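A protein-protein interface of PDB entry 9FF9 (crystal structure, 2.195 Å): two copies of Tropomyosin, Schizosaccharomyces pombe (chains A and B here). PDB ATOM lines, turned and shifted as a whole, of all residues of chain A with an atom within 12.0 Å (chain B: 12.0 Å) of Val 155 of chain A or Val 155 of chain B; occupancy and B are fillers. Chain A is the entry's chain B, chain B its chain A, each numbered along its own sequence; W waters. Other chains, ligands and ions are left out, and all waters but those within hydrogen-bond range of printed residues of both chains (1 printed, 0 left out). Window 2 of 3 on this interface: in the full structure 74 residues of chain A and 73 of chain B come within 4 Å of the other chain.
Of the printed residues of chain B, Tyr 145 of chain A touches Val 148 (3.6 Å).
Of the printed residues of chain B, Val 148 of chain A touches Val 148.
Of the printed residues of chain B, Lys 149 of chain A touches Val 148.
Leu 152 of chain A touches two residues of chain B.
Val 155 of chain A touches just one residue of chain B: Val 155.
No residue of chain B comes within 4 Å of His 156 of chain A.
Thr 146 of chain B touches none of the printed residues of chain A.
Leu 152 of chain B touches just one residue of chain A: Glu 151.
No residue of chain A comes within 4 Å of Glu 154 of chain B.
Val 155 of chain B touches just one residue of chain A: Val 155.
No residue of chain A comes within 4 Å of Ala 158 of chain B.
No residue of chain A comes within 4 Å of Leu 159 of chain B.
The nearest residue of chain B that does not touch Val 155 of chain A is Leu 152 of chain B (4.2 Å).
The nearest residue of chain A that does not touch Val 155 of chain B is Leu 159 of chain A (4.4 Å).
Lys 149 of chain A touches Val 148 of chain B, but with the chains exchanged Val 148 of chain A does not touch Lys 149 of chain B (4.03 Å).
Glu 151 of chain A touches Leu 152 of chain B, and with the chains exchanged Leu 152 of chain A touches Glu 151 of chain B.
Leu 152 of chain A touches Val 148 of chain B, but with the chains exchanged Val 148 of chain A does not touch Leu 152 of chain B (4.4 Å).
Val 155 of chain A touches its own counterpart, Val 155 of chain B.
Of the 7 pairs that touch across the chains among the printed residues, 4 have their exchanged pair printed and touching as well.
NZ of Lys 149 of chain A lies within salt-bridge range of OD1 of Asp 153 of chain A (3.5 Å).
Hydrophobic or aromatic side chains of chain B within 4 Å of the printed part of chain A: Val 148, Leu 152 and Val 155.
Among the printed residues, no Asp or Glu carboxylate lies within 4 Å of a Lys or Arg side-chain nitrogen of the other chain.
Water W1 lies within hydrogen-bond range of the side-chain amino group of Lys 149 of chain A (3.2 Å) and the side-chain carboxylate of Glu 151 of chain B (3.4 Å).
Among the printed residues, pairs that only touch across the chains: Tyr 145 of chain A with Val 148 of chain B (3.6 Å), Val 148 of chain A with Val 148 of chain B (3.7 Å), Lys 149 of chain A with Val 148 of chain B (3.7 Å), Glu 151 of chain A with Leu 152 of chain B (3.6 Å), Leu 152 of chain A with Val 148 of chain B (3.7 Å), Leu 152 of chain A with Glu 151 of chain B (3.5 Å) and Val 155 of chain A with Val 155 of chain B (3.97 Å).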
ATOM      1  N   TYR A 145      31.981 -30.170  -9.588  1.00  0.00           N
ATOM      2  CA  TYR A 145      31.227 -29.686 -10.737  1.00  0.00           C
ATOM      3  C   TYR A 145      30.165 -30.691 -11.156  1.00  0.00           C
ATOM      4  O   TYR A 145      29.021 -30.320 -11.428  1.00  0.00           O
ATOM      5  CB  TYR A 145      32.164 -29.389 -11.909  1.00  0.00           C
ATOM      6  CG  TYR A 145      31.421 -29.215 -13.216  1.00  0.00           C
ATOM      7  CD1 TYR A 145      30.764 -28.029 -13.510  1.00  0.00           C
ATOM      8  CD2 TYR A 145      31.367 -30.243 -14.151  1.00  0.00           C
ATOM      9  CE1 TYR A 145      30.077 -27.868 -14.698  1.00  0.00           C
ATOM     10  CE2 TYR A 145      30.680 -30.091 -15.342  1.00  0.00           C
ATOM     11  CZ  TYR A 145      30.038 -28.902 -15.610  1.00  0.00           C
ATOM     12  OH  TYR A 145      29.355 -28.746 -16.796  1.00  0.00           O
ATOM     13  N   THR A 146      30.535 -31.972 -11.236  1.00  0.00           N
ATOM     14  CA  THR A 146      29.560 -32.993 -11.607  1.00  0.00           C
ATOM     15  C   THR A 146      28.421 -33.048 -10.600  1.00  0.00           C
ATOM     16  O   THR A 146      27.252 -33.161 -10.984  1.00  0.00           O
ATOM     17  CB  THR A 146      30.235 -34.358 -11.725  1.00  0.00           C
ATOM     18  OG1 THR A 146      30.966 -34.636 -10.525  1.00  0.00           O
ATOM     19  CG2 THR A 146      31.181 -34.385 -12.918  1.00  0.00           C
ATOM     20  N   LYS A 147      28.739 -32.940  -9.308  1.00  0.00           N
ATOM     21  CA  LYS A 147      27.699 -32.953  -8.281  1.00  0.00           C
ATOM     22  C   LYS A 147      26.724 -31.794  -8.462  1.00  0.00           C
ATOM     23  O   LYS A 147      25.501 -31.997  -8.525  1.00  0.00           O
ATOM     24  CB  LYS A 147      28.347 -32.900  -6.897  1.00  0.00           C
ATOM     25  CG  LYS A 147      27.371 -32.916  -5.739  1.00  0.00           C
ATOM     26  CD  LYS A 147      28.098 -32.624  -4.436  1.00  0.00           C
ATOM     27  CE  LYS A 147      29.312 -33.527  -4.270  1.00  0.00           C
ATOM     28  NZ  LYS A 147      30.131 -33.152  -3.088  1.00  0.00           N
ATOM     29  N   VAL A 148      27.246 -30.565  -8.544  1.00  0.00           N
ATOM     30  CA  VAL A 148      26.354 -29.412  -8.641  1.00  0.00           C
ATOM     31  C   VAL A 148      25.608 -29.411  -9.968  1.00  0.00           C
ATOM     32  O   VAL A 148      24.457 -28.967 -10.037  1.00  0.00           O
ATOM     33  CB  VAL A 148      27.121 -28.093  -8.424  1.00  0.00           C
ATOM     34  CG1 VAL A 148      27.693 -28.035  -7.014  1.00  0.00           C
ATOM     35  CG2 VAL A 148      28.215 -27.920  -9.463  1.00  0.00           C
ATOM     36  N   LYS A 149      26.222 -29.924 -11.037  1.00  0.00           N
ATOM     37  CA  LYS A 149      25.521 -29.996 -12.312  1.00  0.00           C
ATOM     38  C   LYS A 149      24.401 -31.024 -12.261  1.00  0.00           C
ATOM     39  O   LYS A 149      23.340 -30.820 -12.859  1.00  0.00           O
ATOM     40  CB  LYS A 149      26.505 -30.323 -13.435  1.00  0.00           C
ATOM     41  CG  LYS A 149      25.887 -30.304 -14.824  1.00  0.00           C
ATOM     42  CD  LYS A 149      25.212 -28.972 -15.114  1.00  0.00           C
ATOM     43  CE  LYS A 149      24.607 -28.948 -16.511  1.00  0.00           C
ATOM     44  NZ  LYS A 149      23.868 -27.680 -16.780  1.00  0.00           N
ATOM     45  N   ALA A 150      24.613 -32.131 -11.545  1.00  0.00           N
ATOM     46  CA  ALA A 150      23.539 -33.101 -11.363  1.00  0.00           C
ATOM     47  C   ALA A 150      22.386 -32.492 -10.579  1.00  0.00           C
ATOM     48  O   ALA A 150      21.216 -32.688 -10.926  1.00  0.00           O
ATOM     49  CB  ALA A 150      24.071 -34.348 -10.658  1.00  0.00           C
ATOM     50  N   GLU A 151      22.699 -31.735  -9.525  1.00  0.00           N
ATOM     51  CA  GLU A 151      21.642 -31.070  -8.765  1.00  0.00           C
ATOM     52  C   GLU A 151      20.904 -30.044  -9.623  1.00  0.00           C
ATOM     53  O   GLU A 151      19.676 -29.909  -9.529  1.00  0.00           O
ATOM     54  CB  GLU A 151      22.223 -30.406  -7.518  1.00  0.00           C
ATOM     55  CG  GLU A 151      22.857 -31.375  -6.536  1.00  0.00           C
ATOM     56  CD  GLU A 151      23.175 -30.725  -5.203  1.00  0.00           C
ATOM     57  OE1 GLU A 151      22.627 -29.636  -4.926  1.00  0.00           O
ATOM     58  OE2 GLU A 151      23.970 -31.300  -4.433  1.00  0.00           O
ATOM     59  N   LEU A 152      21.635 -29.319 -10.472  1.00  0.00           N
ATOM     60  CA  LEU A 152      21.001 -28.325 -11.333  1.00  0.00           C
ATOM     61  C   LEU A 152      20.123 -28.985 -12.389  1.00  0.00           C
ATOM     62  O   LEU A 152      19.034 -28.488 -12.695  1.00  0.00           O
ATOM     63  CB  LEU A 152      22.066 -27.445 -11.987  1.00  0.00           C
ATOM     64  CG  LEU A 152      21.562 -26.213 -12.740  1.00  0.00           C
ATOM     65  CD1 LEU A 152      20.722 -25.335 -11.826  1.00  0.00           C
ATOM     66  CD2 LEU A 152      22.723 -25.423 -13.326  1.00  0.00           C
ATOM     67  N   ASP A 153      20.576 -30.099 -12.964  1.00  0.00           N
ATOM     68  CA  ASP A 153      19.733 -30.835 -13.901  1.00  0.00           C
ATOM     69  C   ASP A 153      18.488 -31.368 -13.205  1.00  0.00           C
ATOM     70  O   ASP A 153      17.396 -31.367 -13.786  1.00  0.00           O
ATOM     71  CB  ASP A 153      20.523 -31.978 -14.537  1.00  0.00           C
ATOM     72  CG  ASP A 153      21.652 -31.487 -15.421  1.00  0.00           C
ATOM     73  OD1 ASP A 153      21.740 -30.264 -15.656  1.00  0.00           O
ATOM     74  OD2 ASP A 153      22.456 -32.328 -15.879  1.00  0.00           O
ATOM     75  N   GLU A 154      18.636 -31.814 -11.955  1.00  0.00           N
ATOM     76  CA  GLU A 154      17.484 -32.272 -11.184  1.00  0.00           C
ATOM     77  C   GLU A 154      16.465 -31.154 -11.004  1.00  0.00           C
ATOM     78  O   GLU A 154      15.266 -31.350 -11.237  1.00  0.00           O
ATOM     79  CB  GLU A 154      17.945 -32.808  -9.827  1.00  0.00           C
ATOM     80  CG  GLU A 154      16.813 -33.110  -8.857  1.00  0.00           C
ATOM     81  CD  GLU A 154      17.312 -33.591  -7.508  1.00  0.00           C
ATOM     82  OE1 GLU A 154      18.491 -33.994  -7.418  1.00  0.00           O
ATOM     83  OE2 GLU A 154      16.527 -33.562  -6.538  1.00  0.00           O
ATOM     84  N   VAL A 155      16.924 -29.969 -10.592  1.00  0.00           N
ATOM     85  CA  VAL A 155      15.975 -28.879 -10.375  1.00  0.00           C
ATOM     86  C   VAL A 155      15.385 -28.406 -11.700  1.00  0.00           C
ATOM     87  O   VAL A 155      14.211 -28.026 -11.760  1.00  0.00           O
ATOM     88  CB  VAL A 155      16.620 -27.722  -9.579  1.00  0.00           C
ATOM     89  CG1 VAL A 155      17.758 -27.081 -10.342  1.00  0.00           C
ATOM     90  CG2 VAL A 155      15.580 -26.672  -9.229  1.00  0.00           C
ATOM     91  N   HIS A 156      16.159 -28.462 -12.789  1.00  0.00           N
ATOM     92  CA  HIS A 156      15.625 -28.095 -14.097  1.00  0.00           C
ATOM     93  C   HIS A 156      14.504 -29.040 -14.514  1.00  0.00           C
ATOM     94  O   HIS A 156      13.440 -28.601 -14.967  1.00  0.00           O
ATOM     95  CB  HIS A 156      16.740 -28.098 -15.145  1.00  0.00           C
ATOM     96  CG  HIS A 156      17.595 -26.869 -15.129  1.00  0.00           C
ATOM     97  ND1 HIS A 156      18.526 -26.597 -16.108  1.00  0.00           N
ATOM     98  CD2 HIS A 156      17.659 -25.837 -14.253  1.00  0.00           C
ATOM     99  CE1 HIS A 156      19.126 -25.451 -15.838  1.00  0.00           C
ATOM    100  NE2 HIS A 156      18.619 -24.971 -14.717  1.00  0.00           N
ATOM    101  N   GLN A 157      14.731 -30.347 -14.378  1.00  0.00           N
ATOM    102  CA  GLN A 157      13.700 -31.311 -14.743  1.00  0.00           C
ATOM    103  C   GLN A 157      12.484 -31.187 -13.835  1.00  0.00           C
ATOM    104  O   GLN A 157      11.346 -31.352 -14.289  1.00  0.00           O
ATOM    105  CB  GLN A 157      14.262 -32.730 -14.698  1.00  0.00           C
ATOM    106  CG  GLN A 157      13.339 -33.772 -15.307  1.00  0.00           C
ATOM    107  CD  GLN A 157      13.093 -33.530 -16.781  1.00  0.00           C
ATOM    108  OE1 GLN A 157      14.009 -33.177 -17.524  1.00  0.00           O
ATOM    109  NE2 GLN A 157      11.849 -33.713 -17.212  1.00  0.00           N
ATOM    110  N   ALA A 158      12.700 -30.891 -12.551  1.00  0.00           N
ATOM    111  CA  ALA A 158      11.574 -30.712 -11.641  1.00  0.00           C
ATOM    112  C   ALA A 158      10.754 -29.484 -12.016  1.00  0.00           C
ATOM    113  O   ALA A 158       9.522 -29.495 -11.904  1.00  0.00           O
ATOM    114  CB  ALA A 158      12.072 -30.609 -10.200  1.00  0.00           C
ATOM    115  N   LEU A 159      11.419 -28.416 -12.462  1.00  0.00           N
ATOM    116  CA  LEU A 159      10.695 -27.226 -12.901  1.00  0.00           C
ATOM    117  C   LEU A 159       9.955 -27.483 -14.208  1.00  0.00           C
ATOM    118  O   LEU A 159       8.848 -26.971 -14.411  1.00  0.00           O
ATOM    119  CB  LEU A 159      11.660 -26.052 -13.051  1.00  0.00           C
ATOM    120  CG  LEU A 159      12.263 -25.521 -11.752  1.00  0.00           C
ATOM    121  CD1 LEU A 159      13.371 -24.522 -12.040  1.00  0.00           C
ATOM    122  CD2 LEU A 159      11.184 -24.892 -10.892  1.00  0.00           C
ATOM    123  N   GLU A 160      10.552 -28.270 -15.106  1.00  0.00           N
ATOM    124  CA  GLU A 160       9.876 -28.595 -16.358  1.00  0.00           C
ATOM    125  C   GLU A 160       8.676 -29.505 -16.128  1.00  0.00           C
ATOM    126  O   GLU A 160       7.680 -29.410 -16.856  1.00  0.00           O
ATOM    127  CB  GLU A 160      10.856 -29.244 -17.338  1.00  0.00           C
ATOM    128  CG  GLU A 160      11.948 -28.307 -17.839  1.00  0.00           C
ATOM    129  CD  GLU A 160      12.825 -28.941 -18.905  1.00  0.00           C
ATOM    130  OE1 GLU A 160      12.551 -30.093 -19.305  1.00  0.00           O
ATOM    131  OE2 GLU A 160      13.791 -28.284 -19.346  1.00  0.00           O
ATOM    132  N   ASP A 161       8.742 -30.379 -15.126  1.00  0.00           N
ATOM    133  CA  ASP A 161       7.664 -31.322 -14.853  1.00  0.00           C
ATOM    134  C   ASP A 161       6.497 -30.703 -14.093  1.00  0.00           C
ATOM    135  O   ASP A 161       5.561 -31.429 -13.738  1.00  0.00           O
ATOM    136  CB  ASP A 161       8.205 -32.523 -14.074  1.00  0.00           C
ATOM    137  CG  ASP A 161       9.194 -33.342 -14.879  1.00  0.00           C
ATOM    138  OD1 ASP A 161       9.356 -33.061 -16.085  1.00  0.00           O
ATOM    139  OD2 ASP A 161       9.813 -34.264 -14.305  1.00  0.00           O
ATOM    140  N   LEU A 162       6.519 -29.398 -13.836  1.00  0.00           N
ATOM    141  CA  LEU A 162       5.421 -28.749 -13.125  1.00  0.00           C
ATOM    142  C   LEU A 162       4.179 -28.624 -14.000  1.00  0.00           C
ATOM    143  O   LEU A 162       3.054 -28.758 -13.518  1.00  0.00           O
ATOM    144  CB  LEU A 162       5.841 -27.366 -12.628  1.00  0.00           C
ATOM    145  CG  LEU A 162       6.783 -27.334 -11.426  1.00  0.00           C
ATOM    146  CD1 LEU A 162       6.930 -25.912 -10.923  1.00  0.00           C
ATOM    147  CD2 LEU A 162       6.278 -28.248 -10.323  1.00  0.00           C
ATOM    148  OXT LEU A 162       4.271 -28.386 -15.205  1.00  0.00           O
ATOM    149  N   THR B 146      31.826 -22.763 -10.684  1.00  0.00           N
ATOM    150  CA  THR B 146      31.310 -21.526 -10.106  1.00  0.00           C
ATOM    151  C   THR B 146      30.019 -21.092 -10.789  1.00  0.00           C
ATOM    152  O   THR B 146      29.056 -20.702 -10.118  1.00  0.00           O
ATOM    153  CB  THR B 146      32.364 -20.423 -10.201  1.00  0.00           C
ATOM    154  OG1 THR B 146      33.564 -20.849  -9.545  1.00  0.00           O
ATOM    155  CG2 THR B 146      31.863 -19.145  -9.548  1.00  0.00           C
ATOM    156  N   LYS B 147      29.976 -21.163 -12.123  1.00  0.00           N
ATOM    157  CA  LYS B 147      28.783 -20.739 -12.849  1.00  0.00           C
ATOM    158  C   LYS B 147      27.599 -21.649 -12.548  1.00  0.00           C
ATOM    159  O   LYS B 147      26.464 -21.175 -12.416  1.00  0.00           O
ATOM    160  CB  LYS B 147      29.070 -20.703 -14.350  1.00  0.00           C
ATOM    161  CG  LYS B 147      30.153 -19.710 -14.747  1.00  0.00           C
ATOM    162  CD  LYS B 147      30.680 -19.996 -16.144  1.00  0.00           C
ATOM    163  CE  LYS B 147      31.903 -19.151 -16.460  1.00  0.00           C
ATOM    164  NZ  LYS B 147      32.508 -19.519 -17.772  1.00  0.00           N
ATOM    165  N   VAL B 148      27.839 -22.958 -12.433  1.00  0.00           N
ATOM    166  CA  VAL B 148      26.755 -23.879 -12.102  1.00  0.00           C
ATOM    167  C   VAL B 148      26.311 -23.683 -10.657  1.00  0.00           C
ATOM    168  O   VAL B 148      25.114 -23.727 -10.350  1.00  0.00           O
ATOM    169  CB  VAL B 148      27.183 -25.333 -12.372  1.00  0.00           C
ATOM    170  CG1 VAL B 148      26.078 -26.296 -11.966  1.00  0.00           C
ATOM    171  CG2 VAL B 148      27.528 -25.516 -13.840  1.00  0.00           C
ATOM    172  N   LYS B 149      27.265 -23.466  -9.747  1.00  0.00           N
ATOM    173  CA  LYS B 149      26.900 -23.170  -8.365  1.00  0.00           C
ATOM    174  C   LYS B 149      26.199 -21.823  -8.256  1.00  0.00           C
ATOM    175  O   LYS B 149      25.379 -21.622  -7.353  1.00  0.00           O
ATOM    176  CB  LYS B 149      28.141 -23.203  -7.473  1.00  0.00           C
ATOM    177  CG  LYS B 149      27.841 -23.159  -5.983  1.00  0.00           C
ATOM    178  CD  LYS B 149      26.990 -24.347  -5.551  1.00  0.00           C
ATOM    179  CE  LYS B 149      26.724 -24.321  -4.052  1.00  0.00           C
ATOM    180  NZ  LYS B 149      25.866 -25.456  -3.606  1.00  0.00           N
ATOM    181  N   ALA B 150      26.502 -20.896  -9.167  1.00  0.00           N
ATOM    182  CA  ALA B 150      25.821 -19.606  -9.161  1.00  0.00           C
ATOM    183  C   ALA B 150      24.354 -19.763  -9.531  1.00  0.00           C
ATOM    184  O   ALA B 150      23.471 -19.237  -8.844  1.00  0.00           O
ATOM    185  CB  ALA B 150      26.518 -18.640 -10.119  1.00  0.00           C
ATOM    186  N   GLU B 151      24.073 -20.487 -10.619  1.00  0.00           N
ATOM    187  CA  GLU B 151      22.690 -20.678 -11.041  1.00  0.00           C
ATOM    188  C   GLU B 151      21.902 -21.500 -10.032  1.00  0.00           C
ATOM    189  O   GLU B 151      20.685 -21.324  -9.907  1.00  0.00           O
ATOM    190  CB  GLU B 151      22.638 -21.352 -12.411  1.00  0.00           C
ATOM    191  CG  GLU B 151      23.311 -20.568 -13.524  1.00  0.00           C
ATOM    192  CD  GLU B 151      23.199 -21.261 -14.866  1.00  0.00           C
ATOM    193  OE1 GLU B 151      22.492 -22.285 -14.944  1.00  0.00           O
ATOM    194  OE2 GLU B 151      23.815 -20.784 -15.841  1.00  0.00           O
ATOM    195  N   LEU B 152      22.570 -22.404  -9.317  1.00  0.00           N
ATOM    196  CA  LEU B 152      21.875 -23.230  -8.337  1.00  0.00           C
ATOM    197  C   LEU B 152      21.452 -22.405  -7.129  1.00  0.00           C
ATOM    198  O   LEU B 152      20.301 -22.476  -6.685  1.00  0.00           O
ATOM    199  CB  LEU B 152      22.769 -24.393  -7.910  1.00  0.00           C
ATOM    200  CG  LEU B 152      22.102 -25.469  -7.061  1.00  0.00           C
ATOM    201  CD1 LEU B 152      20.962 -26.120  -7.834  1.00  0.00           C
ATOM    202  CD2 LEU B 152      23.121 -26.506  -6.624  1.00  0.00           C
ATOM    203  N   ASP B 153      22.377 -21.615  -6.582  1.00  0.00           N
ATOM    204  CA  ASP B 153      22.038 -20.744  -5.462  1.00  0.00           C
ATOM    205  C   ASP B 153      21.038 -19.671  -5.871  1.00  0.00           C
ATOM    206  O   ASP B 153      20.260 -19.197  -5.036  1.00  0.00           O
ATOM    207  CB  ASP B 153      23.308 -20.109  -4.899  1.00  0.00           C
ATOM    208  CG  ASP B 153      24.330 -21.143  -4.468  1.00  0.00           C
ATOM    209  OD1 ASP B 153      23.988 -22.345  -4.459  1.00  0.00           O
ATOM    210  OD2 ASP B 153      25.474 -20.761  -4.143  1.00  0.00           O
ATOM    211  N   GLU B 154      21.042 -19.284  -7.148  1.00  0.00           N
ATOM    212  CA  GLU B 154      20.070 -18.315  -7.640  1.00  0.00           C
ATOM    213  C   GLU B 154      18.657 -18.888  -7.623  1.00  0.00           C
ATOM    214  O   GLU B 154      17.713 -18.210  -7.201  1.00  0.00           O
ATOM    215  CB  GLU B 154      20.459 -17.868  -9.048  1.00  0.00           C
ATOM    216  CG  GLU B 154      19.389 -17.100  -9.791  1.00  0.00           C
ATOM    217  CD  GLU B 154      19.795 -16.788 -11.218  1.00  0.00           C
ATOM    218  OE1 GLU B 154      21.012 -16.683 -11.476  1.00  0.00           O
ATOM    219  OE2 GLU B 154      18.902 -16.660 -12.081  1.00  0.00           O
ATOM    220  N   VAL B 155      18.491 -20.134  -8.076  1.00  0.00           N
ATOM    221  CA  VAL B 155      17.174 -20.762  -8.031  1.00  0.00           C
ATOM    222  C   VAL B 155      16.749 -21.006  -6.590  1.00  0.00           C
ATOM    223  O   VAL B 155      15.587 -20.791  -6.225  1.00  0.00           O
ATOM    224  CB  VAL B 155      17.168 -22.069  -8.846  1.00  0.00           C
ATOM    225  CG1 VAL B 155      15.798 -22.729  -8.785  1.00  0.00           C
ATOM    226  CG2 VAL B 155      17.560 -21.801 -10.290  1.00  0.00           C
ATOM    227  N   HIS B 156      17.683 -21.456  -5.748  1.00  0.00           N
ATOM    228  CA  HIS B 156      17.353 -21.730  -4.354  1.00  0.00           C
ATOM    229  C   HIS B 156      16.894 -20.469  -3.633  1.00  0.00           C
ATOM    230  O   HIS B 156      15.962 -20.514  -2.820  1.00  0.00           O
ATOM    231  CB  HIS B 156      18.557 -22.349  -3.646  1.00  0.00           C
ATOM    232  CG  HIS B 156      18.876 -23.738  -4.105  1.00  0.00           C
ATOM    233  ND1 HIS B 156      17.986 -24.506  -4.824  1.00  0.00           N
ATOM    234  CD2 HIS B 156      19.986 -24.497  -3.948  1.00  0.00           C
ATOM    235  CE1 HIS B 156      18.533 -25.679  -5.090  1.00  0.00           C
ATOM    236  NE2 HIS B 156      19.747 -25.699  -4.569  1.00  0.00           N
ATOM    237  N   GLN B 157      17.532 -19.332  -3.920  1.00  0.00           N
ATOM    238  CA  GLN B 157      17.122 -18.083  -3.288  1.00  0.00           C
ATOM    239  C   GLN B 157      15.817 -17.562  -3.872  1.00  0.00           C
ATOM    240  O   GLN B 157      15.059 -16.872  -3.181  1.00  0.00           O
ATOM    241  CB  GLN B 157      18.224 -17.034  -3.433  1.00  0.00           C
ATOM    242  CG  GLN B 157      18.164 -15.931  -2.392  1.00  0.00           C
ATOM    243  CD  GLN B 157      18.590 -16.405  -1.014  1.00  0.00           C
ATOM    244  OE1 GLN B 157      19.112 -17.509  -0.857  1.00  0.00           O
ATOM    245  NE2 GLN B 157      18.371 -15.567  -0.009  1.00  0.00           N
ATOM    246  N   ALA B 158      15.539 -17.877  -5.139  1.00  0.00           N
ATOM    247  CA  ALA B 158      14.282 -17.465  -5.750  1.00  0.00           C
ATOM    248  C   ALA B 158      13.121 -18.334  -5.291  1.00  0.00           C
ATOM    249  O   ALA B 158      11.982 -17.855  -5.226  1.00  0.00           O
ATOM    250  CB  ALA B 158      14.400 -17.503  -7.274  1.00  0.00           C
ATOM    251  N   LEU B 159      13.383 -19.600  -4.965  1.00  0.00           N
ATOM    252  CA  LEU B 159      12.312 -20.475  -4.501  1.00  0.00           C
ATOM    253  C   LEU B 159      11.888 -20.139  -3.079  1.00  0.00           C
ATOM    254  O   LEU B 159      10.723 -20.345  -2.717  1.00  0.00           O
ATOM    255  CB  LEU B 159      12.746 -21.938  -4.599  1.00  0.00           C
ATOM    256  CG  LEU B 159      12.896 -22.489  -6.020  1.00  0.00           C
ATOM    257  CD1 LEU B 159      13.376 -23.929  -5.994  1.00  0.00           C
ATOM    258  CD2 LEU B 159      11.586 -22.369  -6.787  1.00  0.00           C
ATOM    259  N   GLU B 160      12.807 -19.628  -2.258  1.00  0.00           N
ATOM    260  CA  GLU B 160      12.424 -19.189  -0.921  1.00  0.00           C
ATOM    261  C   GLU B 160      11.577 -17.925  -0.969  1.00  0.00           C
ATOM    262  O   GLU B 160      10.668 -17.757  -0.148  1.00  0.00           O
ATOM    263  CB  GLU B 160      13.667 -18.957  -0.061  1.00  0.00           C
ATOM    264  CG  GLU B 160      14.424 -20.224   0.304  1.00  0.00           C
ATOM    265  CD  GLU B 160      15.535 -19.970   1.306  1.00  0.00           C
ATOM    266  OE1 GLU B 160      15.787 -18.792   1.630  1.00  0.00           O
ATOM    267  OE2 GLU B 160      16.153 -20.949   1.774  1.00  0.00           O
ATOM    268  N   ASP B 161      11.850 -17.036  -1.923  1.00  0.00           N
ATOM    269  CA  ASP B 161      11.183 -15.742  -1.979  1.00  0.00           C
ATOM    270  C   ASP B 161       9.802 -15.797  -2.619  1.00  0.00           C
ATOM    271  O   ASP B 161       9.105 -14.778  -2.621  1.00  0.00           O
ATOM    272  CB  ASP B 161      12.054 -14.738  -2.734  1.00  0.00           C
ATOM    273  CG  ASP B 161      13.361 -14.457  -2.025  1.00  0.00           C
ATOM    274  OD1 ASP B 161      13.564 -14.997  -0.918  1.00  0.00           O
ATOM    275  OD2 ASP B 161      14.185 -13.697  -2.575  1.00  0.00           O
ATOM    276  N   LEU B 162       9.388 -16.938  -3.158  1.00  0.00           N
ATOM    277  CA  LEU B 162       8.063 -17.027  -3.761  1.00  0.00           C
ATOM    278  C   LEU B 162       7.007 -17.213  -2.675  1.00  0.00           C
ATOM    279  O   LEU B 162       7.321 -17.607  -1.551  1.00  0.00           O
ATOM    280  CB  LEU B 162       8.003 -18.167  -4.787  1.00  0.00           C
ATOM    281  CG  LEU B 162       7.940 -19.625  -4.322  1.00  0.00           C
ATOM    282  CD1 LEU B 162       6.501 -20.104  -4.168  1.00  0.00           C
ATOM    283  CD2 LEU B 162       8.694 -20.522  -5.290  1.00  0.00           C
ATOM    284  OXT LEU B 162       5.820 -16.967  -2.893  1.00  0.00           O
HETATM  285  O   HOH W   1      24.478 -24.509 -16.512  1.00  0.00           O
